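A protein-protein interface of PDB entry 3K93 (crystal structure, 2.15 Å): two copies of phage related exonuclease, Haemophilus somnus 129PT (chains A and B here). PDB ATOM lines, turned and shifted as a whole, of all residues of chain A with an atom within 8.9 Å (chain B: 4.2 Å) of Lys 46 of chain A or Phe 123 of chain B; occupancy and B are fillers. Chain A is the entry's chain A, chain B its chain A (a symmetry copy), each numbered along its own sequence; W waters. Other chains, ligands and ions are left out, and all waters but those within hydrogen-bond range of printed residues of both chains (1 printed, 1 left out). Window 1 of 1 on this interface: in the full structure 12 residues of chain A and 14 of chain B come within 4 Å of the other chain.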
ATOM      1  N   TYR A   6     -33.825 -17.589 -26.762  1.00  0.00           N
ATOM      2  CA  TYR A   6     -34.194 -17.575 -25.345  1.00  0.00           C
ATOM      3  C   TYR A   6     -35.661 -17.225 -25.262  1.00  0.00           C
ATOM      4  O   TYR A   6     -36.111 -16.230 -25.829  1.00  0.00           O
ATOM      5  CB  TYR A   6     -33.381 -16.576 -24.558  1.00  0.00           C
ATOM      6  CG  TYR A   6     -31.910 -16.920 -24.455  1.00  0.00           C
ATOM      7  CD1 TYR A   6     -31.431 -17.751 -23.458  1.00  0.00           C
ATOM      8  CD2 TYR A   6     -30.989 -16.395 -25.352  1.00  0.00           C
ATOM      9  CE1 TYR A   6     -30.075 -18.054 -23.367  1.00  0.00           C
ATOM     10  CE2 TYR A   6     -29.637 -16.689 -25.250  1.00  0.00           C
ATOM     11  CZ  TYR A   6     -29.196 -17.518 -24.254  1.00  0.00           C
ATOM     12  OH  TYR A   6     -27.868 -17.822 -24.167  1.00  0.00           O
ATOM     13  N   LYS A  38     -39.749  -9.497 -10.517  1.00  0.00           N
ATOM     14  CA  LYS A  38     -38.540  -9.168 -11.272  1.00  0.00           C
ATOM     15  C   LYS A  38     -37.315  -9.893 -10.771  1.00  0.00           C
ATOM     16  O   LYS A  38     -36.513 -10.359 -11.547  1.00  0.00           O
ATOM     17  CB  LYS A  38     -38.290  -7.689 -11.245  1.00  0.00           C
ATOM     18  CG  LYS A  38     -39.288  -6.948 -12.085  1.00  0.00           C
ATOM     19  CD  LYS A  38     -39.335  -5.500 -11.663  1.00  0.00           C
ATOM     20  CE  LYS A  38     -38.567  -4.624 -12.538  1.00  0.00           C
ATOM     21  NZ  LYS A  38     -39.167  -3.215 -12.436  1.00  0.00           N
ATOM     22  N   SER A  39     -37.207 -10.001  -9.466  1.00  0.00           N
ATOM     23  CA  SER A  39     -36.113 -10.725  -8.868  1.00  0.00           C
ATOM     24  C   SER A  39     -36.166 -12.218  -9.283  1.00  0.00           C
ATOM     25  O   SER A  39     -35.145 -12.801  -9.658  1.00  0.00           O
ATOM     26  CB  SER A  39     -36.148 -10.553  -7.350  1.00  0.00           C
ATOM     27  OG  SER A  39     -35.141 -11.343  -6.775  1.00  0.00           O
ATOM     28  N   ALA A  40     -37.351 -12.816  -9.283  1.00  0.00           N
ATOM     29  CA  ALA A  40     -37.489 -14.200  -9.740  1.00  0.00           C
ATOM     30  C   ALA A  40     -37.149 -14.361 -11.231  1.00  0.00           C
ATOM     31  O   ALA A  40     -36.498 -15.330 -11.628  1.00  0.00           O
ATOM     32  CB  ALA A  40     -38.907 -14.749  -9.436  1.00  0.00           C
ATOM     33  N   VAL A  41     -37.603 -13.427 -12.060  1.00  0.00           N
ATOM     34  CA  VAL A  41     -37.328 -13.499 -13.493  1.00  0.00           C
ATOM     35  C   VAL A  41     -35.806 -13.353 -13.776  1.00  0.00           C
ATOM     36  O   VAL A  41     -35.267 -13.975 -14.677  1.00  0.00           O
ATOM     37  CB  VAL A  41     -38.154 -12.422 -14.290  1.00  0.00           C
ATOM     38  CG1 VAL A  41     -37.723 -12.405 -15.796  1.00  0.00           C
ATOM     39  CG2 VAL A  41     -39.725 -12.706 -14.117  1.00  0.00           C
ATOM     40  N   ARG A  42     -35.115 -12.561 -12.977  1.00  0.00           N
ATOM     41  CA  ARG A  42     -33.650 -12.471 -13.117  1.00  0.00           C
ATOM     42  C   ARG A  42     -32.974 -13.802 -12.829  1.00  0.00           C
ATOM     43  O   ARG A  42     -31.978 -14.134 -13.459  1.00  0.00           O
ATOM     44  CB  ARG A  42     -33.088 -11.456 -12.147  1.00  0.00           C
ATOM     45  CG  ARG A  42     -33.316 -10.028 -12.554  1.00  0.00           C
ATOM     46  CD  ARG A  42     -33.003  -9.149 -11.347  1.00  0.00           C
ATOM     47  NE  ARG A  42     -33.584  -7.863 -11.545  1.00  0.00           N
ATOM     48  CZ  ARG A  42     -33.968  -7.045 -10.600  1.00  0.00           C
ATOM     49  NH1 ARG A  42     -33.812  -7.349  -9.318  1.00  0.00           N
ATOM     50  NH2 ARG A  42     -34.487  -5.879 -10.947  1.00  0.00           N
ATOM     51  N   GLU A  43     -33.487 -14.542 -11.851  1.00  0.00           N
ATOM     52  CA  GLU A  43     -32.906 -15.845 -11.547  1.00  0.00           C
ATOM     53  C   GLU A  43     -33.116 -16.804 -12.716  1.00  0.00           C
ATOM     54  O   GLU A  43     -32.228 -17.628 -13.049  1.00  0.00           O
ATOM     55  CB  GLU A  43     -33.509 -16.451 -10.286  1.00  0.00           C
ATOM     56  CG  GLU A  43     -33.167 -15.712  -9.025  1.00  0.00           C
ATOM     57  CD  GLU A  43     -33.785 -16.340  -7.751  1.00  0.00           C
ATOM     58  OE1 GLU A  43     -34.786 -17.055  -7.846  1.00  0.00           O
ATOM     59  OE2 GLU A  43     -33.267 -16.081  -6.652  1.00  0.00           O
ATOM     60  N   MET A  44     -34.280 -16.696 -13.340  1.00  0.00           N
ATOM     61  CA  MET A  44     -34.591 -17.521 -14.497  1.00  0.00           C
ATOM     62  C   MET A  44     -33.685 -17.110 -15.646  1.00  0.00           C
ATOM     63  O   MET A  44     -33.148 -17.975 -16.319  1.00  0.00           O
ATOM     64  CB  MET A  44     -36.076 -17.388 -14.891  1.00  0.00           C
ATOM     65  CG  MET A  44     -37.056 -17.934 -13.818  1.00  0.00           C
ATOM     66  SD  MET A  44     -38.905 -17.276 -14.093  1.00  0.00           S
ATOM     67  CE  MET A  44     -39.668 -17.784 -12.397  1.00  0.00           C
ATOM     68  N   ALA A  45     -33.526 -15.799 -15.890  1.00  0.00           N
ATOM     69  CA  ALA A  45     -32.625 -15.333 -16.948  1.00  0.00           C
ATOM     70  C   ALA A  45     -31.184 -15.831 -16.706  1.00  0.00           C
ATOM     71  O   ALA A  45     -30.550 -16.310 -17.621  1.00  0.00           O
ATOM     72  CB  ALA A  45     -32.659 -13.817 -17.074  1.00  0.00           C
ATOM     73  N   LYS A  46     -30.690 -15.727 -15.473  1.00  0.00           N
ATOM     74  CA  LYS A  46     -29.309 -16.139 -15.179  1.00  0.00           C
ATOM     75  C   LYS A  46     -29.128 -17.668 -15.279  1.00  0.00           C
ATOM     76  O   LYS A  46     -28.041 -18.154 -15.591  1.00  0.00           O
ATOM     77  CB  LYS A  46     -28.865 -15.652 -13.800  1.00  0.00           C
ATOM     78  CG  LYS A  46     -28.703 -14.147 -13.666  1.00  0.00           C
ATOM     79  CD  LYS A  46     -28.139 -13.760 -12.283  1.00  0.00           C
ATOM     80  CE  LYS A  46     -28.420 -12.308 -11.956  1.00  0.00           C
ATOM     81  NZ  LYS A  46     -27.961 -11.945 -10.592  1.00  0.00           N
ATOM     82  N   PHE A  47     -30.162 -18.428 -14.977  1.00  0.00           N
ATOM     83  CA  PHE A  47     -30.075 -19.849 -15.227  1.00  0.00           C
ATOM     84  C   PHE A  47     -29.951 -20.150 -16.718  1.00  0.00           C
ATOM     85  O   PHE A  47     -29.064 -20.908 -17.127  1.00  0.00           O
ATOM     86  CB  PHE A  47     -31.263 -20.630 -14.656  1.00  0.00           C
ATOM     87  CG  PHE A  47     -31.182 -22.088 -14.957  1.00  0.00           C
ATOM     88  CD1 PHE A  47     -30.264 -22.887 -14.286  1.00  0.00           C
ATOM     89  CD2 PHE A  47     -31.953 -22.656 -15.966  1.00  0.00           C
ATOM     90  CE1 PHE A  47     -30.145 -24.261 -14.579  1.00  0.00           C
ATOM     91  CE2 PHE A  47     -31.851 -24.055 -16.293  1.00  0.00           C
ATOM     92  CZ  PHE A  47     -30.960 -24.850 -15.596  1.00  0.00           C
ATOM     93  N   ASP A  48     -30.816 -19.558 -17.537  1.00  0.00           N
ATOM     94  CA  ASP A  48     -30.812 -19.867 -18.980  1.00  0.00           C
ATOM     95  C   ASP A  48     -29.566 -19.298 -19.672  1.00  0.00           C
ATOM     96  O   ASP A  48     -29.085 -19.876 -20.632  1.00  0.00           O
ATOM     97  CB  ASP A  48     -32.057 -19.308 -19.710  1.00  0.00           C
ATOM     98  CG  ASP A  48     -33.357 -19.921 -19.237  1.00  0.00           C
ATOM     99  OD1 ASP A  48     -33.338 -20.977 -18.599  1.00  0.00           O
ATOM    100  OD2 ASP A  48     -34.416 -19.310 -19.500  1.00  0.00           O
ATOM    101  N   LEU A  49     -29.074 -18.142 -19.215  1.00  0.00           N
ATOM    102  CA  LEU A  49     -27.866 -17.548 -19.808  1.00  0.00           C
ATOM    103  C   LEU A  49     -26.609 -18.240 -19.318  1.00  0.00           C
ATOM    104  O   LEU A  49     -25.688 -18.426 -20.075  1.00  0.00           O
ATOM    105  CB  LEU A  49     -27.739 -16.066 -19.440  1.00  0.00           C
ATOM    106  CG  LEU A  49     -28.726 -15.089 -20.081  1.00  0.00           C
ATOM    107  CD1 LEU A  49     -28.867 -13.818 -19.211  1.00  0.00           C
ATOM    108  CD2 LEU A  49     -28.269 -14.808 -21.490  1.00  0.00           C
ATOM    109  N   PHE A  50     -26.542 -18.564 -18.023  1.00  0.00           N
ATOM    110  CA  PHE A  50     -25.256 -18.923 -17.441  1.00  0.00           C
ATOM    111  C   PHE A  50     -25.229 -20.297 -16.808  1.00  0.00           C
ATOM    112  O   PHE A  50     -24.174 -20.748 -16.385  1.00  0.00           O
ATOM    113  CB  PHE A  50     -24.855 -17.880 -16.407  1.00  0.00           C
ATOM    114  CG  PHE A  50     -24.901 -16.457 -16.904  1.00  0.00           C
ATOM    115  CD1 PHE A  50     -24.171 -16.065 -18.009  1.00  0.00           C
ATOM    116  CD2 PHE A  50     -25.624 -15.500 -16.228  1.00  0.00           C
ATOM    117  CE1 PHE A  50     -24.189 -14.774 -18.441  1.00  0.00           C
ATOM    118  CE2 PHE A  50     -25.625 -14.177 -16.652  1.00  0.00           C
ATOM    119  CZ  PHE A  50     -24.933 -13.823 -17.754  1.00  0.00           C
ATOM    120  N   GLY A  51     -26.381 -20.965 -16.746  1.00  0.00           N
ATOM    121  CA  GLY A  51     -26.461 -22.286 -16.140  1.00  0.00           C
ATOM    122  C   GLY A  51     -26.404 -22.241 -14.617  1.00  0.00           C
ATOM    123  O   GLY A  51     -26.191 -23.255 -13.974  1.00  0.00           O
ATOM    124  N   TYR A  52     -26.613 -21.077 -14.027  1.00  0.00           N
ATOM    125  CA  TYR A  52     -26.538 -20.967 -12.576  1.00  0.00           C
ATOM    126  C   TYR A  52     -27.922 -21.204 -11.975  1.00  0.00           C
ATOM    127  O   TYR A  52     -28.876 -20.440 -12.199  1.00  0.00           O
ATOM    128  CB  TYR A  52     -26.010 -19.608 -12.165  1.00  0.00           C
ATOM    129  CG  TYR A  52     -25.965 -19.404 -10.681  1.00  0.00           C
ATOM    130  CD1 TYR A  52     -27.068 -18.925  -9.993  1.00  0.00           C
ATOM    131  CD2 TYR A  52     -24.819 -19.702  -9.953  1.00  0.00           C
ATOM    132  CE1 TYR A  52     -27.024 -18.753  -8.595  1.00  0.00           C
ATOM    133  CE2 TYR A  52     -24.766 -19.506  -8.594  1.00  0.00           C
ATOM    134  CZ  TYR A  52     -25.884 -19.028  -7.923  1.00  0.00           C
ATOM    135  OH  TYR A  52     -25.840 -18.822  -6.558  1.00  0.00           O
ATOM    136  N   ASN A  53     -28.011 -22.270 -11.206  1.00  0.00           N
ATOM    137  CA  ASN A  53     -29.259 -22.681 -10.578  1.00  0.00           C
ATOM    138  C   ASN A  53     -29.292 -22.136  -9.165  1.00  0.00           C
ATOM    139  O   ASN A  53     -28.507 -22.552  -8.321  1.00  0.00           O
ATOM    140  CB  ASN A  53     -29.362 -24.215 -10.554  1.00  0.00           C
ATOM    141  CG  ASN A  53     -30.813 -24.719 -10.346  1.00  0.00           C
ATOM    142  OD1 ASN A  53     -31.723 -23.974  -9.933  1.00  0.00           O
ATOM    143  ND2 ASN A  53     -31.020 -25.977 -10.647  1.00  0.00           N
ATOM    144  N   ALA A  54     -30.191 -21.181  -8.950  1.00  0.00           N
ATOM    145  CA  ALA A  54     -30.360 -20.527  -7.665  1.00  0.00           C
ATOM    146  C   ALA A  54     -30.820 -21.534  -6.609  1.00  0.00           C
ATOM    147  O   ALA A  54     -30.239 -21.587  -5.570  1.00  0.00           O
ATOM    148  CB  ALA A  54     -31.373 -19.372  -7.782  1.00  0.00           C
ATOM    149  N   TYR A 215     -38.057 -10.602 -19.070  1.00  0.00           N
ATOM    150  CA  TYR A 215     -37.021 -11.592 -19.394  1.00  0.00           C
ATOM    151  C   TYR A 215     -36.309 -11.271 -20.718  1.00  0.00           C
ATOM    152  O   TYR A 215     -35.080 -11.280 -20.771  1.00  0.00           O
ATOM    153  CB  TYR A 215     -37.673 -12.998 -19.426  1.00  0.00           C
ATOM    154  CG  TYR A 215     -36.814 -14.180 -19.890  1.00  0.00           C
ATOM    155  CD1 TYR A 215     -36.677 -14.480 -21.237  1.00  0.00           C
ATOM    156  CD2 TYR A 215     -36.154 -15.001 -18.966  1.00  0.00           C
ATOM    157  CE1 TYR A 215     -35.886 -15.577 -21.666  1.00  0.00           C
ATOM    158  CE2 TYR A 215     -35.380 -16.103 -19.379  1.00  0.00           C
ATOM    159  CZ  TYR A 215     -35.272 -16.390 -20.734  1.00  0.00           C
ATOM    160  OH  TYR A 215     -34.543 -17.453 -21.160  1.00  0.00           O
ATOM    161  N   LEU A 218     -33.924  -8.619 -20.337  1.00  0.00           N
ATOM    162  CA  LEU A 218     -32.726  -9.033 -19.613  1.00  0.00           C
ATOM    163  C   LEU A 218     -31.781  -9.744 -20.580  1.00  0.00           C
ATOM    164  O   LEU A 218     -30.586  -9.442 -20.592  1.00  0.00           O
ATOM    165  CB  LEU A 218     -33.051  -9.928 -18.410  1.00  0.00           C
ATOM    166  CG  LEU A 218     -33.878  -9.322 -17.285  1.00  0.00           C
ATOM    167  CD1 LEU A 218     -34.082 -10.360 -16.187  1.00  0.00           C
ATOM    168  CD2 LEU A 218     -33.265  -7.997 -16.695  1.00  0.00           C
ATOM    169  N   ILE A 219     -32.316 -10.661 -21.381  1.00  0.00           N
ATOM    170  CA  ILE A 219     -31.529 -11.401 -22.375  1.00  0.00           C
ATOM    171  C   ILE A 219     -30.812 -10.443 -23.338  1.00  0.00           C
ATOM    172  O   ILE A 219     -29.649 -10.628 -23.619  1.00  0.00           O
ATOM    173  CB  ILE A 219     -32.402 -12.384 -23.189  1.00  0.00           C
ATOM    174  CG1 ILE A 219     -32.986 -13.497 -22.302  1.00  0.00           C
ATOM    175  CG2 ILE A 219     -31.604 -13.015 -24.355  1.00  0.00           C
ATOM    176  CD1 ILE A 219     -31.966 -14.299 -21.474  1.00  0.00           C
ATOM    177  N   GLU A 221     -29.775  -7.418 -22.822  1.00  0.00           N
ATOM    178  CA  GLU A 221     -28.630  -6.762 -22.207  1.00  0.00           C
ATOM    179  C   GLU A 221     -27.367  -7.628 -22.272  1.00  0.00           C
ATOM    180  O   GLU A 221     -26.288  -7.107 -22.224  1.00  0.00           O
ATOM    181  CB  GLU A 221     -28.899  -6.458 -20.729  1.00  0.00           C
ATOM    182  CG  GLU A 221     -29.890  -5.359 -20.483  1.00  0.00           C
ATOM    183  CD  GLU A 221     -29.918  -4.949 -19.019  1.00  0.00           C
ATOM    184  OE1 GLU A 221     -28.851  -4.841 -18.383  1.00  0.00           O
ATOM    185  OE2 GLU A 221     -31.019  -4.731 -18.504  1.00  0.00           O
ATOM    186  N   MET A 222     -27.514  -8.942 -22.315  1.00  0.00           N
ATOM    187  CA  MET A 222     -26.386  -9.837 -22.305  1.00  0.00           C
ATOM    188  C   MET A 222     -26.123 -10.337 -23.725  1.00  0.00           C
ATOM    189  O   MET A 222     -25.669 -11.455 -23.922  1.00  0.00           O
ATOM    190  CB  MET A 222     -26.680 -11.018 -21.370  1.00  0.00           C
ATOM    191  CG  MET A 222     -26.790 -10.632 -19.910  1.00  0.00           C
ATOM    192  SD  MET A 222     -25.111 -10.048 -19.347  1.00  0.00           S
ATOM    193  CE  MET A 222     -25.414  -8.122 -19.122  1.00  0.00           C
ATOM    194  N   ILE B 118     -22.658 -15.807  -9.441  1.00  0.00           N
ATOM    195  CA  ILE B 118     -23.532 -15.370 -10.534  1.00  0.00           C
ATOM    196  C   ILE B 118     -24.866 -14.882  -9.964  1.00  0.00           C
ATOM    197  O   ILE B 118     -25.393 -13.874 -10.389  1.00  0.00           O
ATOM    198  CB  ILE B 118     -23.739 -16.509 -11.587  1.00  0.00           C
ATOM    199  CG1 ILE B 118     -22.412 -16.783 -12.330  1.00  0.00           C
ATOM    200  CG2 ILE B 118     -24.910 -16.188 -12.564  1.00  0.00           C
ATOM    201  CD1 ILE B 118     -22.324 -18.160 -13.022  1.00  0.00           C
ATOM    202  N   GLY B 119     -25.379 -15.592  -8.977  1.00  0.00           N
ATOM    203  CA  GLY B 119     -26.622 -15.204  -8.346  1.00  0.00           C
ATOM    204  C   GLY B 119     -26.638 -13.832  -7.702  1.00  0.00           C
ATOM    205  O   GLY B 119     -27.637 -13.106  -7.826  1.00  0.00           O
ATOM    206  N   HIS B 121     -24.256 -11.440  -8.199  1.00  0.00           N
ATOM    207  CA  HIS B 121     -23.684 -10.434  -9.091  1.00  0.00           C
ATOM    208  C   HIS B 121     -24.773  -9.744  -9.934  1.00  0.00           C
ATOM    209  O   HIS B 121     -25.557 -10.429 -10.580  1.00  0.00           O
ATOM    210  CB  HIS B 121     -22.670 -11.071 -10.038  1.00  0.00           C
ATOM    211  CG  HIS B 121     -22.059 -10.097 -10.979  1.00  0.00           C
ATOM    212  ND1 HIS B 121     -21.137  -9.165 -10.574  1.00  0.00           N
ATOM    213  CD2 HIS B 121     -22.267  -9.875 -12.298  1.00  0.00           C
ATOM    214  CE1 HIS B 121     -20.774  -8.433 -11.611  1.00  0.00           C
ATOM    215  NE2 HIS B 121     -21.466  -8.821 -12.662  1.00  0.00           N
ATOM    216  N   PRO B 122     -24.801  -8.411  -9.947  1.00  0.00           N
ATOM    217  CA  PRO B 122     -25.796  -7.688 -10.738  1.00  0.00           C
ATOM    218  C   PRO B 122     -25.381  -7.463 -12.207  1.00  0.00           C
ATOM    219  O   PRO B 122     -24.795  -6.432 -12.569  1.00  0.00           O
ATOM    220  CB  PRO B 122     -25.932  -6.366 -10.003  1.00  0.00           C
ATOM    221  CG  PRO B 122     -24.593  -6.149  -9.347  1.00  0.00           C
ATOM    222  CD  PRO B 122     -24.003  -7.507  -9.097  1.00  0.00           C
ATOM    223  N   PHE B 123     -25.663  -8.468 -13.024  1.00  0.00           N
ATOM    224  CA  PHE B 123     -25.445  -8.396 -14.424  1.00  0.00           C
ATOM    225  C   PHE B 123     -26.295  -7.310 -15.055  1.00  0.00           C
ATOM    226  O   PHE B 123     -25.847  -6.680 -16.010  1.00  0.00           O
ATOM    227  CB  PHE B 123     -25.808  -9.723 -15.109  1.00  0.00           C
ATOM    228  CG  PHE B 123     -24.810 -10.831 -14.866  1.00  0.00           C
ATOM    229  CD1 PHE B 123     -23.720 -10.990 -15.707  1.00  0.00           C
ATOM    230  CD2 PHE B 123     -24.987 -11.729 -13.827  1.00  0.00           C
ATOM    231  CE1 PHE B 123     -22.797 -12.010 -15.506  1.00  0.00           C
ATOM    232  CE2 PHE B 123     -24.072 -12.733 -13.621  1.00  0.00           C
ATOM    233  CZ  PHE B 123     -22.963 -12.867 -14.480  1.00  0.00           C
ATOM    234  N   PHE B 124     -27.531  -7.124 -14.571  1.00  0.00           N
ATOM    235  CA  PHE B 124     -28.523  -6.325 -15.297  1.00  0.00           C
ATOM    236  C   PHE B 124     -28.512  -4.919 -14.768  1.00  0.00           C
ATOM    237  O   PHE B 124     -28.299  -4.733 -13.606  1.00  0.00           O
ATOM    238  CB  PHE B 124     -29.876  -7.012 -15.196  1.00  0.00           C
ATOM    239  CG  PHE B 124     -29.824  -8.435 -15.686  1.00  0.00           C
ATOM    240  CD1 PHE B 124     -29.529  -8.700 -17.013  1.00  0.00           C
ATOM    241  CD2 PHE B 124     -30.008  -9.505 -14.823  1.00  0.00           C
ATOM    242  CE1 PHE B 124     -29.437 -10.014 -17.466  1.00  0.00           C
ATOM    243  CE2 PHE B 124     -29.930 -10.799 -15.268  1.00  0.00           C
ATOM    244  CZ  PHE B 124     -29.622 -11.057 -16.597  1.00  0.00           C
ATOM    245  N   THR B 125     -28.735  -3.925 -15.623  1.00  0.00           N
ATOM    246  CA  THR B 125     -28.562  -2.544 -15.161  1.00  0.00           C
ATOM    247  C   THR B 125     -29.528  -2.152 -14.040  1.00  0.00           C
ATOM    248  O   THR B 125     -29.080  -1.501 -13.071  1.00  0.00           O
ATOM    249  CB  THR B 125     -28.616  -1.517 -16.286  1.00  0.00           C
ATOM    250  OG1 THR B 125     -29.819  -1.695 -17.040  1.00  0.00           O
ATOM    251  CG2 THR B 125     -27.403  -1.674 -17.182  1.00  0.00           C
ATOM    252  N   GLU B 127     -30.861  -4.184 -11.889  1.00  0.00           N
ATOM    253  CA  GLU B 127     -30.377  -4.976 -10.784  1.00  0.00           C
ATOM    254  C   GLU B 127     -29.198  -4.329 -10.070  1.00  0.00           C
ATOM    255  O   GLU B 127     -29.148  -4.327  -8.835  1.00  0.00           O
ATOM    256  CB  GLU B 127     -29.978  -6.374 -11.286  1.00  0.00           C
ATOM    257  CG  GLU B 127     -29.683  -7.390 -10.175  1.00  0.00           C
ATOM    258  CD  GLU B 127     -29.142  -8.720 -10.718  1.00  0.00           C
ATOM    259  OE1 GLU B 127     -28.807  -8.828 -11.966  1.00  0.00           O
ATOM    260  OE2 GLU B 127     -29.024  -9.638  -9.879  1.00  0.00           O
ATOM    261  N   LEU B 159     -17.472  -9.669 -11.331  1.00  0.00           N
ATOM    262  CA  LEU B 159     -17.554 -11.101 -11.014  1.00  0.00           C
ATOM    263  C   LEU B 159     -16.333 -11.808 -11.553  1.00  0.00           C
ATOM    264  O   LEU B 159     -16.139 -11.896 -12.787  1.00  0.00           O
ATOM    265  CB  LEU B 159     -18.814 -11.744 -11.637  1.00  0.00           C
ATOM    266  CG  LEU B 159     -18.966 -13.234 -11.335  1.00  0.00           C
ATOM    267  CD1 LEU B 159     -19.065 -13.502  -9.811  1.00  0.00           C
ATOM    268  CD2 LEU B 159     -20.166 -13.884 -12.112  1.00  0.00           C
ATOM    269  N   ILE B 183     -18.024 -17.145 -18.957  1.00  0.00           N
ATOM    270  CA  ILE B 183     -18.697 -15.916 -19.328  1.00  0.00           C
ATOM    271  C   ILE B 183     -17.601 -14.951 -19.715  1.00  0.00           C
ATOM    272  O   ILE B 183     -16.679 -14.763 -18.959  1.00  0.00           O
ATOM    273  CB  ILE B 183     -19.503 -15.317 -18.153  1.00  0.00           C
ATOM    274  CG1 ILE B 183     -20.482 -16.335 -17.558  1.00  0.00           C
ATOM    275  CG2 ILE B 183     -20.233 -14.056 -18.562  1.00  0.00           C
ATOM    276  CD1 ILE B 183     -21.161 -15.796 -16.237  1.00  0.00           C
ATOM    277  N   ARG B 187     -18.653  -9.151 -19.994  1.00  0.00           N
ATOM    278  CA  ARG B 187     -20.022  -9.263 -19.452  1.00  0.00           C
ATOM    279  C   ARG B 187     -20.096  -9.386 -17.927  1.00  0.00           C
ATOM    280  O   ARG B 187     -21.206  -9.408 -17.349  1.00  0.00           O
ATOM    281  CB  ARG B 187     -20.753 -10.441 -20.080  1.00  0.00           C
ATOM    282  CG  ARG B 187     -21.151 -10.168 -21.553  1.00  0.00           C
ATOM    283  CD  ARG B 187     -21.509 -11.421 -22.246  1.00  0.00           C
ATOM    284  NE  ARG B 187     -21.813 -11.196 -23.659  1.00  0.00           N
ATOM    285  CZ  ARG B 187     -22.257 -12.138 -24.491  1.00  0.00           C
ATOM    286  NH1 ARG B 187     -22.445 -13.382 -24.066  1.00  0.00           N
ATOM    287  NH2 ARG B 187     -22.512 -11.837 -25.755  1.00  0.00           N
ATOM    288  N   THR B 190     -20.384  -4.650 -14.360  1.00  0.00           N
ATOM    289  CA  THR B 190     -21.502  -3.745 -14.532  1.00  0.00           C
ATOM    290  C   THR B 190     -21.224  -2.545 -13.671  1.00  0.00           C
ATOM    291  O   THR B 190     -20.956  -2.697 -12.466  1.00  0.00           O
ATOM    292  CB  THR B 190     -22.848  -4.371 -14.120  1.00  0.00           C
ATOM    293  OG1 THR B 190     -23.078  -5.538 -14.907  1.00  0.00           O
ATOM    294  CG2 THR B 190     -24.037  -3.388 -14.357  1.00  0.00           C
HETATM  295  O   HOH W   1     -30.430 -13.547  -9.373  1.00  0.00           O
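Of chain B, only Ile 118 (3.2 Å), Gly 119 (3.0 Å), His 121 (2.8 Å), Phe 123 (3.95 Å), Phe 124 (3.9 Å) and Glu 127 (2.6 Å) come within 4 Å of Lys 46 of chain A. Of chain A, only Lys 46 (3.0 Å) and Tyr 52 (3.6 Å) come within 4 Å of Gly 119 of chain B. No residue of chain A comes within 4 Å of Pro 122 of chain B. Of chain A, only Lys 46, Leu 49, Leu 218, Glu 221 and Met 222 come within 4 Å of Phe 124 of chain B. Of the printed residues of chain B, Met 222 of chain A touches Phe 123 (3.5 Å), Phe 124 (3.7 Å) and Arg 187 (3.5 Å). Of the printed residues of chain A, Glu 127 of chain B touches Arg 42 (3.9 Å) and Lys 46 (2.6 Å). Leu 159 of chain B touches none of the printed residues of chain A. The nearest printed residue of chain A that does not touch Glu 127 of chain B is Leu 218 of chain A (6.5 Å).
No position is printed for both chains. Of the 19 pairs that touch across the chains among the printed residues, none has its exchanged pair printed and touching as well.
Glu 127 of chain B touches Arg 42 of chain A. Phe 123 of chain B touches Lys 46 of chain A. Leu 49 of chain A touches Phe 124 of chain B. CG2 of Ile 118 of chain B touches CD2 of Phe 50 of chain A, 3.8 Å away. Phe 50 of chain A touches Phe 123 of chain B. Ile 118 of chain B touches Tyr 52 of chain A (CG2 to CB, 3.6 Å). CA of Gly 119 of chain B touches CE1 of Tyr 52 of chain A, 3.6 Å away. CE1 of Phe 124 of chain B touches O of Leu 218 of chain A (3.4 Å). Glu 221 of chain A touches Phe 124 of chain B (OE1 to CA, 3.4 Å). Met 222 of chain A touches Arg 187 of chain B.
The side-chain amino group (NZ) of Lys 46 of chain A is in hydrogen-bond range of the backbone carbonyl oxygen (O) of Ile 118 of chain B. NZ of Lys 46 of chain A is in hydrogen-bond range of O of Gly 119 of chain B (3.0 Å). The side-chain amino group (NZ) of Lys 46 of chain A lies within hydrogen-bond range of the backbone carbonyl oxygen (O) of His 121 of chain B (2.8 Å). NZ of Lys 46 of chain A lies within salt-bridge range of OE2 of Glu 127 of chain B. The side-chain carboxylate (OE1) of Glu 221 of chain A lies within hydrogen-bond range of the backbone NH (N) of Thr 125 of chain B (2.9 Å).
Of the 12 printed residues of chain B, 9 touch a printed residue of chain A. Hydrophobic or aromatic side chains of chain B within 4 Å of the printed part of chain A: Ile 118, Phe 123, Phe 124 and Ile 183. Of the 23 printed residues of chain A, 8 touch a printed residue of chain B. Printed residues of chain A that touch a printed residue of chain B: Arg 42, Lys 46, Leu 49, Phe 50, Tyr 52, Leu 218, Glu 221 and Met 222.
The backbone carbonyl oxygen of Lys 46 of chain A sits at hydrogen-bond distance from the backbone NH of Gly 51 of chain A. OE1 of Glu 127 of chain B sits at hydrogen-bond distance from N of Phe 123 of chain B (3.3 Å). The side-chain hydroxyl (OG1) of Thr 190 of chain B is in hydrogen-bond range of the backbone carbonyl oxygen (O) of Phe 123 of chain B (3.2 Å). N of Phe 124 of chain B sits close to OE1 of Glu 127 of chain B (3.4 Å).
Water W1 bridges NZ of Lys 46 of chain A and O of Gly 119 of chain B.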
